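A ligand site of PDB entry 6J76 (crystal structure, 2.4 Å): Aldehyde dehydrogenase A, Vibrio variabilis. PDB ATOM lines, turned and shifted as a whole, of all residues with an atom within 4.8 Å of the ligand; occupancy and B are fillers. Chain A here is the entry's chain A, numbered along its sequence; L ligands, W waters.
The backbone carbonyl oxygen of Gly 204 sits at hydrogen-bond distance from the side-chain hydroxyl of Ser 176, 3.2 Å away. The backbone NH (N) of Thr 147 is in hydrogen-bond range of the backbone carbonyl oxygen (O) of Lys 173 (3.4 Å). NZ of Lys 173 lies within hydrogen-bond range of O of Gly 204 (2.7 Å). The backbone NH of Thr 175 lies within hydrogen-bond range of the backbone carbonyl oxygen of Thr 147 (3.3 Å). The backbone carbonyl oxygen (O) of Glu 248 sits at hydrogen-bond distance from the backbone NH (N) of Gly 226. O of Ile 146 is in hydrogen-bond range of N of Thr 225 (2.9 Å). The backbone NH (N) of Glu 248 lies within hydrogen-bond range of the backbone carbonyl oxygen (O) of Met 224 (2.9 Å). The backbone NH of Leu 411 sits at hydrogen-bond distance from the side-chain hydroxyl of Ser 455 (3.3 Å).
Water W6 lies within hydrogen-bond range of an oxygen (O16) of the ligand (2.5 Å) and the side-chain hydroxyl (OG1) of Thr 175 (2.8 Å). Water W1 lies within hydrogen-bond range of the side-chain carboxylate (OE1) of Glu 248, a nitrogen (N7) of the ligand and the backbone carbonyl oxygen (O) of Ser 455. Water W9 lies within hydrogen-bond range of OE1 of Glu 460 (2.4 Å), NH1 of Arg 158 (2.8 Å), OG1 of Thr 225 (2.9 Å) and O14 of the ligand (3.0 Å). Water W10 lies within hydrogen-bond range of the side-chain hydroxyl (OG) of Ser 233 (2.5 Å), the side-chain amide nitrogen (ND2) of Asn 211 (2.8 Å) and a nitrogen (N4) of the ligand (3.2 Å). Water W8 bridges the indole nitrogen of Trp 149 and an oxygen (O8) of the ligand.
An oxygen (O11) of the ligand lies close to the backbone carbonyl oxygen (O) of Gly 226 (3.3 Å). Residues that only touch the ligand: Ile 146, Ala 148, Asn 150, Pro 174, Gly 204, Gly 205, Arg 207, Gly 210, Asn 211, Met 224, Thr 225, Ala 230, Ile 234, Gly 250, Phe 385 and Leu 411. Of the 36 residues printed, 30 come within 4 Å of the ligand.
N of Ser 176 is in hydrogen-bond range of O15 of the ligand. OG of Ser 176 is in hydrogen-bond range of O15 of the ligand. An oxygen (O1) of the ligand lies within hydrogen-bond range of the backbone NH of Ser 227. The side-chain hydroxyl (OG) of Ser 227 lies within hydrogen-bond range of an oxygen (O1) of the ligand (2.7 Å). The side-chain carboxylate (OE1) of Glu 383 sits at hydrogen-bond distance from an oxygen (O12) of the ligand. The backbone NH (N) of Trp 149 lies close to an oxygen (O9) of the ligand, 3.4 Å away. O8 of the ligand sits at hydrogen-bond distance from NE1 of Trp 149 (2.7 Å). A ring nitrogen (NE2) of His 449 lies within hydrogen-bond range of an oxygen (O14) of the ligand. O of Leu 249 sits at hydrogen-bond distance from N7 of the ligand, at 2.8 Å. The side-chain amino group of Lys 173 is in salt-bridge range of an oxygen (O15) of the ligand, 2.8 Å away. The backbone NH (N) of Gly 206 lies within hydrogen-bond range of an oxygen (O17) of the ligand, at 2.8 Å. N3 of the ligand lies within hydrogen-bond range of OG of Ser 233 (2.9 Å). The backbone carbonyl oxygen (O) of Thr 147 sits at hydrogen-bond distance from an oxygen (O5) of the ligand (2.9 Å). The backbone carbonyl oxygen of Glu 248 lies close to a nitrogen (N7) of the ligand (3.3 Å). An oxygen (O5) of the ligand lies close to the backbone NH of Thr 175. O14 of the ligand lies close to SG of Cys 282 (3.5 Å).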
ATOM      1  N   ILE A 146     -10.900  -3.895   1.678  1.00  0.00           N
ATOM      2  CA  ILE A 146     -10.448  -4.023   3.065  1.00  0.00           C
ATOM      3  C   ILE A 146     -10.115  -5.484   3.320  1.00  0.00           C
ATOM      4  O   ILE A 146     -10.918  -6.367   2.986  1.00  0.00           O
ATOM      5  CB  ILE A 146     -11.531  -3.499   4.028  1.00  0.00           C
ATOM      6  CG1 ILE A 146     -11.837  -2.024   3.719  1.00  0.00           C
ATOM      7  CG2 ILE A 146     -11.124  -3.659   5.471  1.00  0.00           C
ATOM      8  CD1 ILE A 146     -12.856  -1.368   4.642  1.00  0.00           C
ATOM      9  N   THR A 147      -8.919  -5.753   3.857  1.00  0.00           N
ATOM     10  CA  THR A 147      -8.438  -7.127   4.009  1.00  0.00           C
ATOM     11  C   THR A 147      -8.218  -7.481   5.475  1.00  0.00           C
ATOM     12  O   THR A 147      -8.107  -6.609   6.336  1.00  0.00           O
ATOM     13  CB  THR A 147      -7.115  -7.364   3.236  1.00  0.00           C
ATOM     14  OG1 THR A 147      -6.079  -6.535   3.775  1.00  0.00           O
ATOM     15  CG2 THR A 147      -7.277  -7.078   1.754  1.00  0.00           C
ATOM     16  N   ALA A 148      -8.127  -8.786   5.729  1.00  0.00           N
ATOM     17  CA  ALA A 148      -7.890  -9.377   7.047  1.00  0.00           C
ATOM     18  C   ALA A 148      -6.453  -9.883   7.133  1.00  0.00           C
ATOM     19  O   ALA A 148      -5.739  -9.970   6.128  1.00  0.00           O
ATOM     20  CB  ALA A 148      -8.879 -10.517   7.310  1.00  0.00           C
ATOM     21  N   TRP A 149      -6.008 -10.229   8.339  1.00  0.00           N
ATOM     22  CA  TRP A 149      -4.579 -10.480   8.548  1.00  0.00           C
ATOM     23  C   TRP A 149      -4.149 -11.930   8.304  1.00  0.00           C
ATOM     24  O   TRP A 149      -2.936 -12.185   8.305  1.00  0.00           O
ATOM     25  CB  TRP A 149      -4.149 -10.038   9.968  1.00  0.00           C
ATOM     26  CG  TRP A 149      -5.001 -10.585  11.096  1.00  0.00           C
ATOM     27  CD1 TRP A 149      -5.921  -9.882  11.823  1.00  0.00           C
ATOM     28  CD2 TRP A 149      -4.991 -11.919  11.629  1.00  0.00           C
ATOM     29  NE1 TRP A 149      -6.499 -10.712  12.768  1.00  0.00           N
ATOM     30  CE2 TRP A 149      -5.950 -11.961  12.658  1.00  0.00           C
ATOM     31  CE3 TRP A 149      -4.276 -13.075  11.321  1.00  0.00           C
ATOM     32  CZ2 TRP A 149      -6.218 -13.124  13.395  1.00  0.00           C
ATOM     33  CZ3 TRP A 149      -4.545 -14.241  12.044  1.00  0.00           C
ATOM     34  CH2 TRP A 149      -5.508 -14.248  13.074  1.00  0.00           C
ATOM     35  N   ASN A 150      -5.062 -12.881   8.070  1.00  0.00           N
ATOM     36  CA  ASN A 150      -4.623 -14.273   8.045  1.00  0.00           C
ATOM     37  C   ASN A 150      -4.009 -14.661   6.717  1.00  0.00           C
ATOM     38  O   ASN A 150      -3.142 -15.543   6.673  1.00  0.00           O
ATOM     39  CB  ASN A 150      -5.776 -15.213   8.399  1.00  0.00           C
ATOM     40  CG  ASN A 150      -6.878 -15.223   7.340  1.00  0.00           C
ATOM     41  OD1 ASN A 150      -7.204 -14.197   6.744  1.00  0.00           O
ATOM     42  ND2 ASN A 150      -7.461 -16.388   7.119  1.00  0.00           N
ATOM     43  N   LEU A 155      -5.648 -11.893  -0.097  1.00  0.00           N
ATOM     44  CA  LEU A 155      -6.917 -11.183  -0.028  1.00  0.00           C
ATOM     45  C   LEU A 155      -6.866  -9.901  -0.831  1.00  0.00           C
ATOM     46  O   LEU A 155      -7.858  -9.519  -1.483  1.00  0.00           O
ATOM     47  CB  LEU A 155      -7.283 -10.890   1.428  1.00  0.00           C
ATOM     48  CG  LEU A 155      -7.630 -12.139   2.224  1.00  0.00           C
ATOM     49  CD1 LEU A 155      -7.942 -11.725   3.670  1.00  0.00           C
ATOM     50  CD2 LEU A 155      -8.801 -12.884   1.575  1.00  0.00           C
ATOM     51  N   ARG A 158      -7.089 -11.106  -4.451  1.00  0.00           N
ATOM     52  CA  ARG A 158      -8.444 -11.598  -4.682  1.00  0.00           C
ATOM     53  C   ARG A 158      -9.402 -10.473  -5.046  1.00  0.00           C
ATOM     54  O   ARG A 158     -10.435 -10.714  -5.699  1.00  0.00           O
ATOM     55  CB  ARG A 158      -8.916 -12.330  -3.417  1.00  0.00           C
ATOM     56  CG  ARG A 158     -10.366 -12.740  -3.390  1.00  0.00           C
ATOM     57  CD  ARG A 158     -10.665 -13.481  -2.101  1.00  0.00           C
ATOM     58  NE  ARG A 158     -11.197 -14.819  -2.347  1.00  0.00           N
ATOM     59  CZ  ARG A 158     -11.381 -15.735  -1.406  1.00  0.00           C
ATOM     60  NH1 ARG A 158     -11.075 -15.451  -0.149  1.00  0.00           N
ATOM     61  NH2 ARG A 158     -11.871 -16.936  -1.721  1.00  0.00           N
ATOM     62  N   LYS A 173      -7.327  -0.830   1.686  1.00  0.00           N
ATOM     63  CA  LYS A 173      -6.940  -0.603   3.077  1.00  0.00           C
ATOM     64  C   LYS A 173      -6.604  -1.938   3.718  1.00  0.00           C
ATOM     65  O   LYS A 173      -7.509  -2.682   4.127  1.00  0.00           O
ATOM     66  CB  LYS A 173      -8.021   0.115   3.879  1.00  0.00           C
ATOM     67  CG  LYS A 173      -7.460   0.627   5.236  1.00  0.00           C
ATOM     68  CD  LYS A 173      -8.341   0.322   6.432  1.00  0.00           C
ATOM     69  CE  LYS A 173      -8.161  -1.074   6.976  1.00  0.00           C
ATOM     70  NZ  LYS A 173      -7.189  -1.143   8.093  1.00  0.00           N
ATOM     71  N   PRO A 174      -5.326  -2.293   3.825  1.00  0.00           N
ATOM     72  CA  PRO A 174      -4.979  -3.562   4.461  1.00  0.00           C
ATOM     73  C   PRO A 174      -5.170  -3.527   5.966  1.00  0.00           C
ATOM     74  O   PRO A 174      -5.160  -2.465   6.603  1.00  0.00           O
ATOM     75  CB  PRO A 174      -3.501  -3.752   4.089  1.00  0.00           C
ATOM     76  CG  PRO A 174      -2.995  -2.399   3.755  1.00  0.00           C
ATOM     77  CD  PRO A 174      -4.161  -1.557   3.309  1.00  0.00           C
ATOM     78  N   THR A 175      -5.400  -4.712   6.527  1.00  0.00           N
ATOM     79  CA  THR A 175      -5.330  -4.924   7.973  1.00  0.00           C
ATOM     80  C   THR A 175      -4.093  -4.234   8.554  1.00  0.00           C
ATOM     81  O   THR A 175      -3.000  -4.287   7.990  1.00  0.00           O
ATOM     82  CB  THR A 175      -5.273  -6.428   8.265  1.00  0.00           C
ATOM     83  OG1 THR A 175      -5.002  -6.639   9.653  1.00  0.00           O
ATOM     84  CG2 THR A 175      -4.177  -7.105   7.440  1.00  0.00           C
ATOM     85  N   SER A 176      -4.281  -3.578   9.701  1.00  0.00           N
ATOM     86  CA  SER A 176      -3.147  -2.938  10.357  1.00  0.00           C
ATOM     87  C   SER A 176      -2.216  -3.960  11.010  1.00  0.00           C
ATOM     88  O   SER A 176      -1.072  -3.618  11.320  1.00  0.00           O
ATOM     89  CB  SER A 176      -3.632  -1.948  11.410  1.00  0.00           C
ATOM     90  OG  SER A 176      -4.484  -0.981  10.832  1.00  0.00           O
ATOM     91  N   GLY A 204      -4.418   2.379   8.192  1.00  0.00           N
ATOM     92  CA  GLY A 204      -5.066   3.074   9.295  1.00  0.00           C
ATOM     93  C   GLY A 204      -6.132   2.210   9.908  1.00  0.00           C
ATOM     94  O   GLY A 204      -6.447   1.114   9.414  1.00  0.00           O
ATOM     95  N   GLY A 205      -6.695   2.713  11.005  1.00  0.00           N
ATOM     96  CA  GLY A 205      -7.677   1.928  11.746  1.00  0.00           C
ATOM     97  C   GLY A 205      -8.936   1.693  10.940  1.00  0.00           C
ATOM     98  O   GLY A 205      -9.481   2.618  10.313  1.00  0.00           O
ATOM     99  N   GLY A 206      -9.403   0.446  10.929  1.00  0.00           N
ATOM    100  CA  GLY A 206     -10.671   0.152  10.278  1.00  0.00           C
ATOM    101  C   GLY A 206     -11.824   0.986  10.792  1.00  0.00           C
ATOM    102  O   GLY A 206     -12.732   1.327  10.018  1.00  0.00           O
ATOM    103  N   ARG A 207     -11.810   1.345  12.069  1.00  0.00           N
ATOM    104  CA  ARG A 207     -12.946   2.055  12.643  1.00  0.00           C
ATOM    105  C   ARG A 207     -12.890   3.549  12.367  1.00  0.00           C
ATOM    106  O   ARG A 207     -13.901   4.238  12.563  1.00  0.00           O
ATOM    107  CB  ARG A 207     -13.052   1.819  14.151  1.00  0.00           C
ATOM    108  CG  ARG A 207     -13.445   0.374  14.495  1.00  0.00           C
ATOM    109  CD  ARG A 207     -13.980   0.240  15.925  1.00  0.00           C
ATOM    110  NE  ARG A 207     -14.630   1.468  16.370  1.00  0.00           N
ATOM    111  CZ  ARG A 207     -15.895   1.576  16.772  1.00  0.00           C
ATOM    112  NH1 ARG A 207     -16.676   0.501  16.778  1.00  0.00           N
ATOM    113  NH2 ARG A 207     -16.377   2.745  17.171  1.00  0.00           N
ATOM    114  N   GLY A 210     -11.056   3.175   7.631  1.00  0.00           N
ATOM    115  CA  GLY A 210     -11.899   2.223   6.928  1.00  0.00           C
ATOM    116  C   GLY A 210     -13.368   2.601   6.954  1.00  0.00           C
ATOM    117  O   GLY A 210     -14.050   2.539   5.935  1.00  0.00           O
ATOM    118  N   ASN A 211     -13.867   3.010   8.127  1.00  0.00           N
ATOM    119  CA  ASN A 211     -15.275   3.398   8.237  1.00  0.00           C
ATOM    120  C   ASN A 211     -15.591   4.611   7.367  1.00  0.00           C
ATOM    121  O   ASN A 211     -16.675   4.704   6.785  1.00  0.00           O
ATOM    122  CB  ASN A 211     -15.622   3.693   9.691  1.00  0.00           C
ATOM    123  CG  ASN A 211     -17.014   4.282   9.849  1.00  0.00           C
ATOM    124  OD1 ASN A 211     -17.160   5.480  10.135  1.00  0.00           O
ATOM    125  ND2 ASN A 211     -18.034   3.460   9.639  1.00  0.00           N
ATOM    126  N   VAL A 214     -15.719   3.412   3.522  1.00  0.00           N
ATOM    127  CA  VAL A 214     -16.826   2.595   3.024  1.00  0.00           C
ATOM    128  C   VAL A 214     -18.136   3.364   2.930  1.00  0.00           C
ATOM    129  O   VAL A 214     -18.986   2.999   2.114  1.00  0.00           O
ATOM    130  CB  VAL A 214     -17.040   1.340   3.886  1.00  0.00           C
ATOM    131  CG1 VAL A 214     -15.757   0.541   3.950  1.00  0.00           C
ATOM    132  CG2 VAL A 214     -17.509   1.718   5.289  1.00  0.00           C
ATOM    133  N   MET A 224     -14.794  -6.427   1.155  1.00  0.00           N
ATOM    134  CA  MET A 224     -14.152  -6.483   2.449  1.00  0.00           C
ATOM    135  C   MET A 224     -14.181  -7.908   2.985  1.00  0.00           C
ATOM    136  O   MET A 224     -15.171  -8.631   2.850  1.00  0.00           O
ATOM    137  CB  MET A 224     -14.827  -5.516   3.434  1.00  0.00           C
ATOM    138  CG  MET A 224     -14.382  -5.665   4.868  1.00  0.00           C
ATOM    139  SD  MET A 224     -15.426  -6.800   5.793  1.00  0.00           S
ATOM    140  CE  MET A 224     -14.747  -6.608   7.442  1.00  0.00           C
ATOM    141  N   THR A 225     -13.059  -8.298   3.581  1.00  0.00           N
ATOM    142  CA  THR A 225     -12.913  -9.551   4.285  1.00  0.00           C
ATOM    143  C   THR A 225     -12.536  -9.242   5.731  1.00  0.00           C
ATOM    144  O   THR A 225     -11.714  -8.365   5.987  1.00  0.00           O
ATOM    145  CB  THR A 225     -11.824 -10.386   3.621  1.00  0.00           C
ATOM    146  OG1 THR A 225     -12.260 -10.762   2.317  1.00  0.00           O
ATOM    147  CG2 THR A 225     -11.528 -11.613   4.435  1.00  0.00           C
ATOM    148  N   GLY A 226     -13.149  -9.959   6.683  1.00  0.00           N
ATOM    149  CA  GLY A 226     -12.855  -9.713   8.084  1.00  0.00           C
ATOM    150  C   GLY A 226     -13.914 -10.338   8.988  1.00  0.00           C
ATOM    151  O   GLY A 226     -14.671 -11.203   8.564  1.00  0.00           O
ATOM    152  N   SER A 227     -13.944  -9.873  10.245  1.00  0.00           N
ATOM    153  CA  SER A 227     -14.872 -10.403  11.247  1.00  0.00           C
ATOM    154  C   SER A 227     -16.300  -9.928  10.994  1.00  0.00           C
ATOM    155  O   SER A 227     -16.547  -8.887  10.388  1.00  0.00           O
ATOM    156  CB  SER A 227     -14.449  -9.987  12.651  1.00  0.00           C
ATOM    157  OG  SER A 227     -14.534  -8.573  12.808  1.00  0.00           O
ATOM    158  N   ALA A 230     -17.241  -6.344  12.249  1.00  0.00           N
ATOM    159  CA  ALA A 230     -16.751  -5.280  11.373  1.00  0.00           C
ATOM    160  C   ALA A 230     -17.621  -5.164  10.132  1.00  0.00           C
ATOM    161  O   ALA A 230     -17.925  -4.047   9.692  1.00  0.00           O
ATOM    162  CB  ALA A 230     -15.296  -5.534  10.986  1.00  0.00           C
ATOM    163  N   SER A 233     -20.753  -3.327  10.830  1.00  0.00           N
ATOM    164  CA  SER A 233     -20.522  -1.891  10.847  1.00  0.00           C
ATOM    165  C   SER A 233     -20.455  -1.319   9.447  1.00  0.00           C
ATOM    166  O   SER A 233     -20.935  -0.213   9.188  1.00  0.00           O
ATOM    167  CB  SER A 233     -19.242  -1.583  11.639  1.00  0.00           C
ATOM    168  OG  SER A 233     -18.670  -0.367  11.231  1.00  0.00           O
ATOM    169  N   ILE A 234     -19.885  -2.087   8.509  1.00  0.00           N
ATOM    170  CA  ILE A 234     -19.805  -1.620   7.122  1.00  0.00           C
ATOM    171  C   ILE A 234     -21.185  -1.592   6.480  1.00  0.00           C
ATOM    172  O   ILE A 234     -21.523  -0.657   5.729  1.00  0.00           O
ATOM    173  CB  ILE A 234     -18.806  -2.483   6.340  1.00  0.00           C
ATOM    174  CG1 ILE A 234     -17.389  -2.268   6.898  1.00  0.00           C
ATOM    175  CG2 ILE A 234     -18.878  -2.191   4.828  1.00  0.00           C
ATOM    176  CD1 ILE A 234     -16.309  -3.037   6.207  1.00  0.00           C
ATOM    177  N   GLU A 248     -17.142 -10.646   3.310  1.00  0.00           N
ATOM    178  CA  GLU A 248     -16.798 -12.046   3.532  1.00  0.00           C
ATOM    179  C   GLU A 248     -16.315 -12.166   4.982  1.00  0.00           C
ATOM    180  O   GLU A 248     -15.174 -11.813   5.275  1.00  0.00           O
ATOM    181  CB  GLU A 248     -15.713 -12.506   2.563  1.00  0.00           C
ATOM    182  CG  GLU A 248     -16.002 -12.409   1.053  1.00  0.00           C
ATOM    183  CD  GLU A 248     -17.467 -12.544   0.638  1.00  0.00           C
ATOM    184  OE1 GLU A 248     -18.139 -13.532   1.016  1.00  0.00           O
ATOM    185  OE2 GLU A 248     -17.917 -11.682  -0.150  1.00  0.00           O
ATOM    186  N   LEU A 249     -17.165 -12.705   5.848  1.00  0.00           N
ATOM    187  CA  LEU A 249     -17.016 -12.501   7.286  1.00  0.00           C
ATOM    188  C   LEU A 249     -16.699 -13.833   7.991  1.00  0.00           C
ATOM    189  O   LEU A 249     -15.999 -14.685   7.430  1.00  0.00           O
ATOM    190  CB  LEU A 249     -18.265 -11.782   7.793  1.00  0.00           C
ATOM    191  CG  LEU A 249     -18.591 -10.579   6.881  1.00  0.00           C
ATOM    192  CD1 LEU A 249     -19.923  -9.959   7.198  1.00  0.00           C
ATOM    193  CD2 LEU A 249     -17.467  -9.505   6.898  1.00  0.00           C
ATOM    194  N   GLY A 250     -17.155 -13.986   9.230  1.00  0.00           N
ATOM    195  CA  GLY A 250     -16.675 -15.075  10.069  1.00  0.00           C
ATOM    196  C   GLY A 250     -17.239 -16.421   9.652  1.00  0.00           C
ATOM    197  O   GLY A 250     -18.151 -16.539   8.838  1.00  0.00           O
ATOM    198  N   GLY A 251     -16.678 -17.472  10.253  1.00  0.00           N
ATOM    199  CA  GLY A 251     -17.159 -18.812  10.001  1.00  0.00           C
ATOM    200  C   GLY A 251     -17.164 -19.658  11.260  1.00  0.00           C
ATOM    201  O   GLY A 251     -16.537 -19.328  12.270  1.00  0.00           O
ATOM    202  N   CYS A 282     -10.863 -18.925   7.397  1.00  0.00           N
ATOM    203  CA  CYS A 282     -12.290 -18.688   7.565  1.00  0.00           C
ATOM    204  C   CYS A 282     -13.130 -19.916   7.233  1.00  0.00           C
ATOM    205  O   CYS A 282     -14.345 -19.910   7.489  1.00  0.00           O
ATOM    206  CB  CYS A 282     -12.730 -17.530   6.684  1.00  0.00           C
ATOM    207  SG  CYS A 282     -12.694 -17.977   4.919  1.00  0.00           S
ATOM    208  N   GLU A 383     -16.762 -18.183  17.119  1.00  0.00           N
ATOM    209  CA  GLU A 383     -15.597 -18.454  16.280  1.00  0.00           C
ATOM    210  C   GLU A 383     -14.316 -18.311  17.083  1.00  0.00           C
ATOM    211  O   GLU A 383     -14.122 -17.333  17.801  1.00  0.00           O
ATOM    212  CB  GLU A 383     -15.586 -17.494  15.085  1.00  0.00           C
ATOM    213  CG  GLU A 383     -14.473 -17.784  14.070  1.00  0.00           C
ATOM    214  CD  GLU A 383     -14.314 -16.691  13.008  1.00  0.00           C
ATOM    215  OE1 GLU A 383     -14.599 -15.510  13.297  1.00  0.00           O
ATOM    216  OE2 GLU A 383     -13.991 -17.061  11.856  1.00  0.00           O
ATOM    217  N   PHE A 385     -10.975 -19.249  15.563  1.00  0.00           N
ATOM    218  CA  PHE A 385      -9.945 -18.801  14.628  1.00  0.00           C
ATOM    219  C   PHE A 385      -8.559 -19.129  15.176  1.00  0.00           C
ATOM    220  O   PHE A 385      -7.624 -18.333  15.088  1.00  0.00           O
ATOM    221  CB  PHE A 385     -10.091 -17.310  14.324  1.00  0.00           C
ATOM    222  CG  PHE A 385      -9.648 -16.926  12.939  1.00  0.00           C
ATOM    223  CD1 PHE A 385     -10.233 -17.523  11.829  1.00  0.00           C
ATOM    224  CD2 PHE A 385      -8.689 -15.936  12.748  1.00  0.00           C
ATOM    225  CE1 PHE A 385      -9.844 -17.163  10.543  1.00  0.00           C
ATOM    226  CE2 PHE A 385      -8.281 -15.570  11.475  1.00  0.00           C
ATOM    227  CZ  PHE A 385      -8.856 -16.166  10.365  1.00  0.00           C
ATOM    228  N   LEU A 411     -20.756 -20.370   6.329  1.00  0.00           N
ATOM    229  CA  LEU A 411     -19.808 -20.336   5.222  1.00  0.00           C
ATOM    230  C   LEU A 411     -19.456 -21.754   4.792  1.00  0.00           C
ATOM    231  O   LEU A 411     -20.075 -22.292   3.858  1.00  0.00           O
ATOM    232  CB  LEU A 411     -18.549 -19.544   5.603  1.00  0.00           C
ATOM    233  CG  LEU A 411     -17.438 -19.432   4.568  1.00  0.00           C
ATOM    234  CD1 LEU A 411     -17.979 -19.077   3.173  1.00  0.00           C
ATOM    235  CD2 LEU A 411     -16.409 -18.402   5.025  1.00  0.00           C
ATOM    236  N   HIS A 449     -17.138 -18.387  -3.342  1.00  0.00           N
ATOM    237  CA  HIS A 449     -16.877 -18.356  -1.900  1.00  0.00           C
ATOM    238  C   HIS A 449     -17.989 -17.509  -1.273  1.00  0.00           C
ATOM    239  O   HIS A 449     -17.933 -16.283  -1.281  1.00  0.00           O
ATOM    240  CB  HIS A 449     -15.484 -17.770  -1.658  1.00  0.00           C
ATOM    241  CG  HIS A 449     -15.043 -17.805  -0.232  1.00  0.00           C
ATOM    242  ND1 HIS A 449     -14.828 -18.979   0.457  1.00  0.00           N
ATOM    243  CD2 HIS A 449     -14.717 -16.805   0.619  1.00  0.00           C
ATOM    244  CE1 HIS A 449     -14.420 -18.710   1.681  1.00  0.00           C
ATOM    245  NE2 HIS A 449     -14.343 -17.390   1.806  1.00  0.00           N
ATOM    246  N   SER A 455     -22.146 -14.873   7.860  1.00  0.00           N
ATOM    247  CA  SER A 455     -20.848 -15.120   7.241  1.00  0.00           C
ATOM    248  C   SER A 455     -20.588 -14.217   6.029  1.00  0.00           C
ATOM    249  O   SER A 455     -19.501 -14.305   5.442  1.00  0.00           O
ATOM    250  CB  SER A 455     -20.721 -16.594   6.821  1.00  0.00           C
ATOM    251  OG  SER A 455     -20.485 -17.458   7.933  1.00  0.00           O
ATOM    252  N   GLU A 460     -17.702 -14.241  -3.153  1.00  0.00           N
ATOM    253  CA  GLU A 460     -16.483 -13.794  -3.807  1.00  0.00           C
ATOM    254  C   GLU A 460     -15.983 -14.884  -4.747  1.00  0.00           C
ATOM    255  O   GLU A 460     -16.355 -16.056  -4.621  1.00  0.00           O
ATOM    256  CB  GLU A 460     -15.423 -13.454  -2.741  1.00  0.00           C
ATOM    257  CG  GLU A 460     -14.461 -12.362  -3.117  1.00  0.00           C
ATOM    258  CD  GLU A 460     -13.600 -11.861  -1.945  1.00  0.00           C
ATOM    259  OE1 GLU A 460     -13.617 -12.481  -0.859  1.00  0.00           O
ATOM    260  OE2 GLU A 460     -12.887 -10.844  -2.127  1.00  0.00           O
HETATM  261  P1  LIG L   1     -11.131  -7.659  11.506  1.00  0.00           P
HETATM  262  O1  LIG L   1     -12.602  -7.459  11.364  1.00  0.00           O
HETATM  263  O2  LIG L   1     -10.615  -7.495  12.937  1.00  0.00           O
HETATM  264  O3  LIG L   1     -10.426  -6.643  10.539  1.00  0.00           O
HETATM  265  C1  LIG L   1     -10.819  -6.572   9.192  1.00  0.00           C
HETATM  266  C2  LIG L   1     -10.495  -5.379   8.420  1.00  0.00           C
HETATM  267  O4  LIG L   1     -11.592  -4.428   8.486  1.00  0.00           O
HETATM  268  C3  LIG L   1      -9.317  -4.710   8.934  1.00  0.00           C
HETATM  269  O5  LIG L   1      -8.553  -4.175   7.880  1.00  0.00           O
HETATM  270  C4  LIG L   1      -9.841  -3.687   9.807  1.00  0.00           C
HETATM  271  O6  LIG L   1      -8.989  -2.649  10.047  1.00  0.00           O
HETATM  272  C5  LIG L   1     -11.201  -3.321   9.245  1.00  0.00           C
HETATM  273  N1  LIG L   1     -12.088  -3.037  10.376  1.00  0.00           N
HETATM  274  C6  LIG L   1     -12.383  -3.265  11.645  1.00  0.00           C
HETATM  275  N2  LIG L   1     -13.476  -2.493  11.796  1.00  0.00           N
HETATM  276  C7  LIG L   1     -13.796  -1.852  10.641  1.00  0.00           C
HETATM  277  C8  LIG L   1     -14.814  -0.959  10.322  1.00  0.00           C
HETATM  278  N3  LIG L   1     -15.785  -0.589  11.351  1.00  0.00           N
HETATM  279  N4  LIG L   1     -14.885  -0.472   9.060  1.00  0.00           N
HETATM  280  C9  LIG L   1     -13.974  -0.833   8.116  1.00  0.00           C
HETATM  281  N5  LIG L   1     -12.980  -1.688   8.428  1.00  0.00           N
HETATM  282  C10 LIG L   1     -12.865  -2.211   9.660  1.00  0.00           C
HETATM  283  O7  LIG L   1     -10.841  -9.089  10.977  1.00  0.00           O
HETATM  284  P2  LIG L   1      -9.418  -9.779  11.134  1.00  0.00           P
HETATM  285  O8  LIG L   1      -9.125  -9.923  12.589  1.00  0.00           O
HETATM  286  O9  LIG L   1      -8.368  -8.975  10.411  1.00  0.00           O
HETATM  287  O10 LIG L   1      -9.493 -11.210  10.512  1.00  0.00           O
HETATM  288  C11 LIG L   1     -10.168 -12.282  11.172  1.00  0.00           C
HETATM  289  C12 LIG L   1     -11.559 -12.528  10.735  1.00  0.00           C
HETATM  290  O11 LIG L   1     -11.648 -12.401   9.320  1.00  0.00           O
HETATM  291  C13 LIG L   1     -11.982 -13.887  11.092  1.00  0.00           C
HETATM  292  O12 LIG L   1     -13.300 -13.810  11.673  1.00  0.00           O
HETATM  293  C14 LIG L   1     -12.057 -14.559   9.854  1.00  0.00           C
HETATM  294  O13 LIG L   1     -13.074 -15.521   9.852  1.00  0.00           O
HETATM  295  C15 LIG L   1     -12.377 -13.486   8.903  1.00  0.00           C
HETATM  296  N6  LIG L   1     -12.130 -13.853   7.520  1.00  0.00           N
HETATM  297  C16 LIG L   1     -13.158 -14.032   6.545  1.00  0.00           C
HETATM  298  C17 LIG L   1     -12.834 -14.530   5.187  1.00  0.00           C
HETATM  299  C18 LIG L   1     -13.875 -14.907   4.322  1.00  0.00           C
HETATM  300  O14 LIG L   1     -13.628 -15.083   3.139  1.00  0.00           O
HETATM  301  N7  LIG L   1     -15.180 -15.104   4.790  1.00  0.00           N
HETATM  302  C19 LIG L   1     -11.437 -14.875   4.816  1.00  0.00           C
HETATM  303  C20 LIG L   1     -10.390 -14.520   5.822  1.00  0.00           C
HETATM  304  C21 LIG L   1     -10.756 -14.012   7.193  1.00  0.00           C
HETATM  305  P3  LIG L   1      -7.948  -2.696  11.195  1.00  0.00           P
HETATM  306  O15 LIG L   1      -6.631  -2.298  10.631  1.00  0.00           O
HETATM  307  O16 LIG L   1      -7.769  -4.097  11.677  1.00  0.00           O
HETATM  308  O17 LIG L   1      -8.266  -1.732  12.369  1.00  0.00           O
HETATM  309  O   HOH W   1     -17.597 -15.430   3.106  1.00  0.00           O
HETATM  310  O   HOH W   2     -10.096  -4.605  13.363  1.00  0.00           O
HETATM  311  O   HOH W   3      -6.018  -0.588  14.269  1.00  0.00           O
HETATM  312  O   HOH W   4     -11.509 -10.629  14.609  1.00  0.00           O
HETATM  313  O   HOH W   5      -6.161  -4.199  13.946  1.00  0.00           O
HETATM  314  O   HOH W   6      -7.313  -6.482  11.312  1.00  0.00           O
HETATM  315  O   HOH W   7      -7.866  -7.519  13.940  1.00  0.00           O
HETATM  316  O   HOH W   8      -7.964 -10.485  15.639  1.00  0.00           O
HETATM  317  O   HOH W   9     -12.415 -13.337   1.059  1.00  0.00           O
HETATM  318  O   HOH W  10     -17.827   0.714   9.157  1.00  0.00           O
